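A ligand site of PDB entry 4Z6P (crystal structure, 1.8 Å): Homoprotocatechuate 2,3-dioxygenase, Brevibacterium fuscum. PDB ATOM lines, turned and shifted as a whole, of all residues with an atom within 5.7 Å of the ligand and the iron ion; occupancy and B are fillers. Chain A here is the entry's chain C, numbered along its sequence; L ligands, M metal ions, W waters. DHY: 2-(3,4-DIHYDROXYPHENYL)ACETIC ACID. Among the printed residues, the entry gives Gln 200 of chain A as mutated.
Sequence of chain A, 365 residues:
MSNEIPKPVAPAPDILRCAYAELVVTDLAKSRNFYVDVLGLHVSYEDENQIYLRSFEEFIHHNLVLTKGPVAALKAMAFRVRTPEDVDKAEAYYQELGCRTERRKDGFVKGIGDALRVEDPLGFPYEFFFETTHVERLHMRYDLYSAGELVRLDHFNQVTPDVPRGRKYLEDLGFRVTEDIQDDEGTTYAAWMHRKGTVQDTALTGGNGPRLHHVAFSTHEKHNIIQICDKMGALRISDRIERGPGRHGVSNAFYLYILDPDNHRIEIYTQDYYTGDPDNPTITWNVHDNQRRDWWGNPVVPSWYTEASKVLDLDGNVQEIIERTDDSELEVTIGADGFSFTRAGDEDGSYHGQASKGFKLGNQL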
ATOM      1  N   HIS A 155      21.731  26.739 -32.332  1.00  0.00           N
ATOM      2  CA  HIS A 155      20.783  27.841 -32.502  1.00  0.00           C
ATOM      3  C   HIS A 155      21.351  29.204 -32.221  1.00  0.00           C
ATOM      4  O   HIS A 155      22.471  29.338 -31.690  1.00  0.00           O
ATOM      5  CB  HIS A 155      19.524  27.617 -31.601  1.00  0.00           C
ATOM      6  CG  HIS A 155      19.801  27.615 -30.130  1.00  0.00           C
ATOM      7  ND1 HIS A 155      20.085  26.463 -29.423  1.00  0.00           N
ATOM      8  CD2 HIS A 155      19.774  28.607 -29.203  1.00  0.00           C
ATOM      9  CE1 HIS A 155      20.230  26.737 -28.138  1.00  0.00           C
ATOM     10  NE2 HIS A 155      20.074  28.036 -27.989  1.00  0.00           N
ATOM     11  N   ASN A 157      19.962  33.026 -30.346  1.00  0.00           N
ATOM     12  CA  ASN A 157      18.964  33.654 -29.504  1.00  0.00           C
ATOM     13  C   ASN A 157      19.098  35.182 -29.609  1.00  0.00           C
ATOM     14  O   ASN A 157      20.171  35.759 -29.435  1.00  0.00           O
ATOM     15  CB  ASN A 157      19.060  33.134 -28.066  1.00  0.00           C
ATOM     16  CG  ASN A 157      17.898  33.607 -27.175  1.00  0.00           C
ATOM     17  OD1 ASN A 157      17.651  34.801 -27.061  1.00  0.00           O
ATOM     18  ND2 ASN A 157      17.180  32.654 -26.572  1.00  0.00           N
ATOM     19  N   ILE A 181       7.217  31.441 -22.888  1.00  0.00           N
ATOM     20  CA  ILE A 181       6.994  31.854 -21.519  1.00  0.00           C
ATOM     21  C   ILE A 181       6.050  33.047 -21.513  1.00  0.00           C
ATOM     22  O   ILE A 181       6.293  34.036 -22.234  1.00  0.00           O
ATOM     23  CB  ILE A 181       8.311  32.273 -20.824  1.00  0.00           C
ATOM     24  CG1 ILE A 181       9.237  31.072 -20.705  1.00  0.00           C
ATOM     25  CG2 ILE A 181       7.989  32.828 -19.428  1.00  0.00           C
ATOM     26  CD1 ILE A 181      10.637  31.399 -20.216  1.00  0.00           C
ATOM     27  N   TRP A 192      10.553  30.177 -28.522  1.00  0.00           N
ATOM     28  CA  TRP A 192      11.586  29.348 -29.139  1.00  0.00           C
ATOM     29  C   TRP A 192      10.973  28.828 -30.423  1.00  0.00           C
ATOM     30  O   TRP A 192       9.828  28.420 -30.413  1.00  0.00           O
ATOM     31  CB  TRP A 192      11.900  28.173 -28.203  1.00  0.00           C
ATOM     32  CG  TRP A 192      12.777  28.564 -27.041  1.00  0.00           C
ATOM     33  CD1 TRP A 192      14.077  28.292 -26.926  1.00  0.00           C
ATOM     34  CD2 TRP A 192      12.408  29.271 -25.838  1.00  0.00           C
ATOM     35  NE1 TRP A 192      14.600  28.823 -25.744  1.00  0.00           N
ATOM     36  CE2 TRP A 192      13.594  29.435 -25.058  1.00  0.00           C
ATOM     37  CE3 TRP A 192      11.208  29.800 -25.343  1.00  0.00           C
ATOM     38  CZ2 TRP A 192      13.587  30.050 -23.814  1.00  0.00           C
ATOM     39  CZ3 TRP A 192      11.217  30.426 -24.111  1.00  0.00           C
ATOM     40  CH2 TRP A 192      12.400  30.558 -23.363  1.00  0.00           C
ATOM     41  N   GLN A 200      14.774  24.494 -31.483  1.00  0.00           N
ATOM     42  CA  GLN A 200      15.037  25.845 -31.936  1.00  0.00           C
ATOM     43  C   GLN A 200      16.134  25.912 -33.006  1.00  0.00           C
ATOM     44  O   GLN A 200      17.155  25.228 -32.936  1.00  0.00           O
ATOM     45  CB  GLN A 200      15.420  26.695 -30.733  1.00  0.00           C
ATOM     46  CG  GLN A 200      16.546  26.076 -29.901  1.00  0.00           C
ATOM     47  CD  GLN A 200      16.816  26.825 -28.626  1.00  0.00           C
ATOM     48  OE1 GLN A 200      17.076  26.219 -27.535  1.00  0.00           O
ATOM     49  NE2 GLN A 200      16.745  28.131 -28.709  1.00  0.00           N
ATOM     50  N   HIS A 214      22.760  35.052 -27.582  1.00  0.00           N
ATOM     51  CA  HIS A 214      23.855  34.084 -27.674  1.00  0.00           C
ATOM     52  C   HIS A 214      23.873  33.283 -28.940  1.00  0.00           C
ATOM     53  O   HIS A 214      22.904  33.306 -29.732  1.00  0.00           O
ATOM     54  CB  HIS A 214      23.839  33.111 -26.477  1.00  0.00           C
ATOM     55  CG  HIS A 214      22.557  32.353 -26.303  1.00  0.00           C
ATOM     56  ND1 HIS A 214      21.528  32.834 -25.525  1.00  0.00           N
ATOM     57  CD2 HIS A 214      22.141  31.153 -26.756  1.00  0.00           C
ATOM     58  CE1 HIS A 214      20.555  31.960 -25.488  1.00  0.00           C
ATOM     59  NE2 HIS A 214      20.889  30.928 -26.232  1.00  0.00           N
ATOM     60  N   ALA A 216      24.554  29.148 -29.759  1.00  0.00           N
ATOM     61  CA  ALA A 216      24.618  27.876 -29.049  1.00  0.00           C
ATOM     62  C   ALA A 216      25.209  26.765 -29.895  1.00  0.00           C
ATOM     63  O   ALA A 216      24.804  26.570 -31.031  1.00  0.00           O
ATOM     64  CB  ALA A 216      23.245  27.443 -28.599  1.00  0.00           C
ATOM     65  N   ARG A 243      26.598  31.419 -16.253  1.00  0.00           N
ATOM     66  CA  ARG A 243      25.388  30.795 -15.706  1.00  0.00           C
ATOM     67  C   ARG A 243      25.396  29.306 -16.061  1.00  0.00           C
ATOM     68  O   ARG A 243      25.675  28.943 -17.184  1.00  0.00           O
ATOM     69  CB  ARG A 243      24.133  31.468 -16.258  1.00  0.00           C
ATOM     70  CG  ARG A 243      22.840  30.682 -16.073  1.00  0.00           C
ATOM     71  CD  ARG A 243      21.548  31.433 -16.420  1.00  0.00           C
ATOM     72  NE  ARG A 243      20.470  30.469 -16.291  1.00  0.00           N
ATOM     73  CZ  ARG A 243      19.486  30.286 -17.172  1.00  0.00           C
ATOM     74  NH1 ARG A 243      19.301  31.104 -18.217  1.00  0.00           N
ATOM     75  NH2 ARG A 243      18.674  29.252 -17.019  1.00  0.00           N
ATOM     76  N   HIS A 248      17.701  22.857 -18.464  1.00  0.00           N
ATOM     77  CA  HIS A 248      16.649  23.801 -18.831  1.00  0.00           C
ATOM     78  C   HIS A 248      15.267  23.195 -18.531  1.00  0.00           C
ATOM     79  O   HIS A 248      15.052  21.985 -18.710  1.00  0.00           O
ATOM     80  CB  HIS A 248      16.664  24.138 -20.319  1.00  0.00           C
ATOM     81  CG  HIS A 248      17.729  25.092 -20.759  1.00  0.00           C
ATOM     82  ND1 HIS A 248      17.924  26.325 -20.159  1.00  0.00           N
ATOM     83  CD2 HIS A 248      18.599  25.039 -21.794  1.00  0.00           C
ATOM     84  CE1 HIS A 248      18.871  26.984 -20.814  1.00  0.00           C
ATOM     85  NE2 HIS A 248      19.314  26.215 -21.792  1.00  0.00           N
ATOM     86  N   GLY A 249      14.327  24.035 -18.156  1.00  0.00           N
ATOM     87  CA  GLY A 249      12.913  23.682 -18.243  1.00  0.00           C
ATOM     88  C   GLY A 249      12.460  23.682 -19.675  1.00  0.00           C
ATOM     89  O   GLY A 249      12.274  22.620 -20.298  1.00  0.00           O
ATOM     90  N   VAL A 250      12.330  24.888 -20.223  1.00  0.00           N
ATOM     91  CA  VAL A 250      12.156  25.067 -21.645  1.00  0.00           C
ATOM     92  C   VAL A 250      13.264  24.331 -22.389  1.00  0.00           C
ATOM     93  O   VAL A 250      14.429  24.551 -22.117  1.00  0.00           O
ATOM     94  CB  VAL A 250      12.188  26.541 -22.055  1.00  0.00           C
ATOM     95  CG1 VAL A 250      12.121  26.678 -23.562  1.00  0.00           C
ATOM     96  CG2 VAL A 250      11.035  27.317 -21.413  1.00  0.00           C
ATOM     97  N   SER A 251      12.874  23.452 -23.291  1.00  0.00           N
ATOM     98  CA  SER A 251      13.791  22.639 -24.137  1.00  0.00           C
ATOM     99  C   SER A 251      14.243  21.328 -23.519  1.00  0.00           C
ATOM    100  O   SER A 251      14.662  20.429 -24.233  1.00  0.00           O
ATOM    101  CB  SER A 251      15.010  23.397 -24.642  1.00  0.00           C
ATOM    102  OG  SER A 251      16.085  23.406 -23.682  1.00  0.00           O
ATOM    103  N   TYR A 255      22.721  22.494 -20.167  1.00  0.00           N
ATOM    104  CA  TYR A 255      23.222  23.793 -20.683  1.00  0.00           C
ATOM    105  C   TYR A 255      24.314  24.417 -19.846  1.00  0.00           C
ATOM    106  O   TYR A 255      24.480  24.088 -18.699  1.00  0.00           O
ATOM    107  CB  TYR A 255      22.101  24.818 -20.834  1.00  0.00           C
ATOM    108  CG  TYR A 255      21.622  25.404 -19.524  1.00  0.00           C
ATOM    109  CD1 TYR A 255      22.204  26.548 -19.004  1.00  0.00           C
ATOM    110  CD2 TYR A 255      20.586  24.823 -18.796  1.00  0.00           C
ATOM    111  CE1 TYR A 255      21.773  27.081 -17.804  1.00  0.00           C
ATOM    112  CE2 TYR A 255      20.152  25.361 -17.586  1.00  0.00           C
ATOM    113  CZ  TYR A 255      20.756  26.495 -17.090  1.00  0.00           C
ATOM    114  OH  TYR A 255      20.310  27.017 -15.877  1.00  0.00           O
ATOM    115  N   TYR A 257      26.217  28.681 -19.984  1.00  0.00           N
ATOM    116  CA  TYR A 257      26.551  29.919 -20.671  1.00  0.00           C
ATOM    117  C   TYR A 257      27.898  30.474 -20.241  1.00  0.00           C
ATOM    118  O   TYR A 257      28.190  30.598 -19.024  1.00  0.00           O
ATOM    119  CB  TYR A 257      25.499  31.011 -20.407  1.00  0.00           C
ATOM    120  CG  TYR A 257      24.132  30.609 -20.813  1.00  0.00           C
ATOM    121  CD1 TYR A 257      23.694  30.811 -22.119  1.00  0.00           C
ATOM    122  CD2 TYR A 257      23.286  30.014 -19.927  1.00  0.00           C
ATOM    123  CE1 TYR A 257      22.433  30.418 -22.510  1.00  0.00           C
ATOM    124  CE2 TYR A 257      22.011  29.655 -20.281  1.00  0.00           C
ATOM    125  CZ  TYR A 257      21.598  29.824 -21.575  1.00  0.00           C
ATOM    126  OH  TYR A 257      20.306  29.446 -21.901  1.00  0.00           O
ATOM    127  N   GLU A 267      26.351  29.610 -25.614  1.00  0.00           N
ATOM    128  CA  GLU A 267      25.697  28.529 -24.882  1.00  0.00           C
ATOM    129  C   GLU A 267      26.247  27.194 -25.366  1.00  0.00           C
ATOM    130  O   GLU A 267      26.478  26.994 -26.583  1.00  0.00           O
ATOM    131  CB  GLU A 267      24.154  28.585 -25.081  1.00  0.00           C
ATOM    132  CG  GLU A 267      23.443  27.472 -24.294  1.00  0.00           C
ATOM    133  CD  GLU A 267      21.939  27.507 -24.448  1.00  0.00           C
ATOM    134  OE1 GLU A 267      21.433  28.173 -25.367  1.00  0.00           O
ATOM    135  OE2 GLU A 267      21.253  26.900 -23.611  1.00  0.00           O
ATOM    136  N   TYR A 269      25.013  23.116 -25.113  1.00  0.00           N
ATOM    137  CA  TYR A 269      23.648  22.644 -25.081  1.00  0.00           C
ATOM    138  C   TYR A 269      23.627  21.193 -25.544  1.00  0.00           C
ATOM    139  O   TYR A 269      24.342  20.814 -26.491  1.00  0.00           O
ATOM    140  CB  TYR A 269      22.845  23.555 -26.003  1.00  0.00           C
ATOM    141  CG  TYR A 269      21.376  23.354 -26.250  1.00  0.00           C
ATOM    142  CD1 TYR A 269      20.940  22.511 -27.277  1.00  0.00           C
ATOM    143  CD2 TYR A 269      20.441  24.115 -25.581  1.00  0.00           C
ATOM    144  CE1 TYR A 269      19.581  22.406 -27.572  1.00  0.00           C
ATOM    145  CE2 TYR A 269      19.092  24.000 -25.880  1.00  0.00           C
ATOM    146  CZ  TYR A 269      18.674  23.155 -26.853  1.00  0.00           C
ATOM    147  OH  TYR A 269      17.326  23.139 -27.177  1.00  0.00           O
ATOM    148  N   ARG A 292      11.218  26.975 -14.865  1.00  0.00           N
ATOM    149  CA  ARG A 292      10.979  27.166 -16.301  1.00  0.00           C
ATOM    150  C   ARG A 292      12.295  27.344 -17.082  1.00  0.00           C
ATOM    151  O   ARG A 292      12.377  26.987 -18.256  1.00  0.00           O
ATOM    152  CB  ARG A 292      10.051  28.365 -16.548  1.00  0.00           C
ATOM    153  CG  ARG A 292      10.749  29.722 -16.454  1.00  0.00           C
ATOM    154  CD  ARG A 292       9.842  30.937 -16.333  1.00  0.00           C
ATOM    155  NE  ARG A 292      10.713  32.094 -16.146  1.00  0.00           N
ATOM    156  CZ  ARG A 292      11.351  32.425 -15.016  1.00  0.00           C
ATOM    157  NH1 ARG A 292      11.171  31.713 -13.904  1.00  0.00           N
ATOM    158  NH2 ARG A 292      12.164  33.475 -14.980  1.00  0.00           N
ATOM    159  N   ARG A 293      13.290  27.941 -16.422  1.00  0.00           N
ATOM    160  CA  ARG A 293      14.535  28.280 -17.049  1.00  0.00           C
ATOM    161  C   ARG A 293      15.584  27.289 -16.556  1.00  0.00           C
ATOM    162  O   ARG A 293      16.078  26.499 -17.335  1.00  0.00           O
ATOM    163  CB  ARG A 293      14.927  29.749 -16.828  1.00  0.00           C
ATOM    164  CG  ARG A 293      14.129  30.675 -17.721  1.00  0.00           C
ATOM    165  CD  ARG A 293      14.757  32.046 -17.932  1.00  0.00           C
ATOM    166  NE  ARG A 293      13.992  32.911 -18.855  1.00  0.00           N
ATOM    167  CZ  ARG A 293      14.120  32.954 -20.187  1.00  0.00           C
ATOM    168  NH1 ARG A 293      14.937  32.149 -20.848  1.00  0.00           N
ATOM    169  NH2 ARG A 293      13.406  33.815 -20.895  1.00  0.00           N
ATOM    170  N   ASP A 294      15.870  27.289 -15.268  1.00  0.00           N
ATOM    171  CA  ASP A 294      16.641  26.203 -14.698  1.00  0.00           C
ATOM    172  C   ASP A 294      15.667  25.300 -14.001  1.00  0.00           C
ATOM    173  O   ASP A 294      14.981  25.709 -13.049  1.00  0.00           O
ATOM    174  CB  ASP A 294      17.696  26.731 -13.733  1.00  0.00           C
ATOM    175  CG  ASP A 294      18.659  25.668 -13.288  1.00  0.00           C
ATOM    176  OD1 ASP A 294      19.615  25.379 -14.066  1.00  0.00           O
ATOM    177  OD2 ASP A 294      18.471  25.126 -12.157  1.00  0.00           O
ATOM    178  N   VAL A 300      18.543  32.706 -11.937  1.00  0.00           N
ATOM    179  CA  VAL A 300      19.095  33.265 -13.172  1.00  0.00           C
ATOM    180  C   VAL A 300      19.763  34.592 -12.808  1.00  0.00           C
ATOM    181  O   VAL A 300      19.102  35.487 -12.339  1.00  0.00           O
ATOM    182  CB  VAL A 300      17.985  33.492 -14.211  1.00  0.00           C
ATOM    183  CG1 VAL A 300      18.516  34.165 -15.485  1.00  0.00           C
ATOM    184  CG2 VAL A 300      17.266  32.169 -14.512  1.00  0.00           C
ATOM    185  N   TRP A 304      22.258  37.844 -17.245  1.00  0.00           N
ATOM    186  CA  TRP A 304      21.679  36.996 -18.290  1.00  0.00           C
ATOM    187  C   TRP A 304      20.497  37.704 -18.939  1.00  0.00           C
ATOM    188  O   TRP A 304      20.254  37.599 -20.128  1.00  0.00           O
ATOM    189  CB  TRP A 304      21.229  35.641 -17.719  1.00  0.00           C
ATOM    190  CG  TRP A 304      21.093  34.620 -18.786  1.00  0.00           C
ATOM    191  CD1 TRP A 304      22.077  33.834 -19.278  1.00  0.00           C
ATOM    192  CD2 TRP A 304      19.922  34.327 -19.555  1.00  0.00           C
ATOM    193  NE1 TRP A 304      21.588  33.029 -20.270  1.00  0.00           N
ATOM    194  CE2 TRP A 304      20.267  33.300 -20.460  1.00  0.00           C
ATOM    195  CE3 TRP A 304      18.616  34.814 -19.558  1.00  0.00           C
ATOM    196  CZ2 TRP A 304      19.365  32.776 -21.381  1.00  0.00           C
ATOM    197  CZ3 TRP A 304      17.731  34.292 -20.463  1.00  0.00           C
ATOM    198  CH2 TRP A 304      18.119  33.282 -21.374  1.00  0.00           C
HETATM  199  C1  DHY L   1      16.202  28.498 -22.152  1.00  0.00           C
HETATM  200  C2  DHY L   1      17.215  29.409 -22.621  1.00  0.00           C
HETATM  201  C3  DHY L   1      18.027  29.022 -23.707  1.00  0.00           C
HETATM  202  C4  DHY L   1      17.771  27.726 -24.342  1.00  0.00           C
HETATM  203  C5  DHY L   1      16.729  26.885 -23.903  1.00  0.00           C
HETATM  204  C6  DHY L   1      15.978  27.256 -22.780  1.00  0.00           C
HETATM  205  C7  DHY L   1      15.608  28.721 -20.769  1.00  0.00           C
HETATM  206  C8  DHY L   1      16.679  29.160 -19.732  1.00  0.00           C
HETATM  207  O1  DHY L   1      17.142  28.345 -18.926  1.00  0.00           O
HETATM  208  O2  DHY L   1      16.974  30.262 -19.730  1.00  0.00           O
HETATM  209  O3  DHY L   1      19.023  29.836 -24.146  1.00  0.00           O
HETATM  210  O4  DHY L   1      18.562  27.321 -25.414  1.00  0.00           O
HETATM  211 FE    FE M   1      19.716  28.978 -25.974  1.00  0.00          FE
HETATM  212  O   HOH W   1      17.698  29.911 -26.874  1.00  0.00           O
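O of Arg 293 sits close to O1 of the ligand (2.7 Å). O2 of the ligand is in salt-bridge range of NH1 of Arg 293 (3.0 Å). An oxygen (O3) of the ligand sits close to the side-chain hydroxyl (OH) of Tyr 257 (2.6 Å). The guanidinium group (NH2) of Arg 243 lies within salt-bridge range of an oxygen (O1) of the ligand (2.6 Å). ND1 of His 248 is in hydrogen-bond range of O1 of the ligand (2.5 Å). An oxygen (O4) of the ligand lies close to the side-chain amide oxygen (OE1) of Gln 200, 2.8 Å away.
The backbone carbonyl oxygen (O) of His 155 is in hydrogen-bond range of the backbone NH (N) of Ala 216. OH of Tyr 257 sits close to NE2 of His 248 (3.4 Å). OH of Tyr 269 is in hydrogen-bond range of OE1 of Gln 200 (3.1 Å). O of His 214 is in hydrogen-bond range of N of Asn 157, at 3.0 Å. OH of Tyr 257 is in hydrogen-bond range of OE2 of Glu 267 (3.2 Å). The guanidinium group (NH2) of Arg 243 lies within hydrogen-bond range of the side-chain hydroxyl (OH) of Tyr 255 (3.0 Å). NE2 of His 155 lies close to NE2 of Gln 200 (3.4 Å). O of Arg 292 is in hydrogen-bond range of N of Val 250.
NE1 of Trp 192 touches C5 of the ligand, 3.4 Å away. O of Val 250 touches C6 of the ligand, at 3.2 Å. OG of Ser 251 touches C5 of the ligand (3.5 Å). Tyr 269 touches the ligand (CE2 to O4, 3.4 Å). CH2 of Trp 304 touches O2 of the ligand, 3.6 Å away. Hydrophobic or aromatic side chains within 4 Å of the ligand: His 155, Trp 192, His 214, His 248, Val 250, Tyr 257, Tyr 269 and Trp 304. Of the 21 residues printed, 13 come within 4 Å of the ligand. The nearest printed residue that does not touch the ligand is Asp 294 (4.01 Å).
Three residues have an atom within 4 Å of the iron ion: His 155, His 214 and Glu 267. The nearest printed residue that does not touch the iron ion is Gln 200 (4.1 Å).
The iron ion is bound by the side-chain carboxylate (OE1) of Glu 267 (2.0 Å), an oxygen (O4) of the ligand (2.1 Å), an oxygen (O3) of the ligand (2.1 Å), a ring nitrogen (NE2) of His 155 (2.3 Å), a ring nitrogen (NE2) of His 214 (2.3 Å) and water W1 (2.4 Å). The iron ion has six donor atoms within binding distance.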
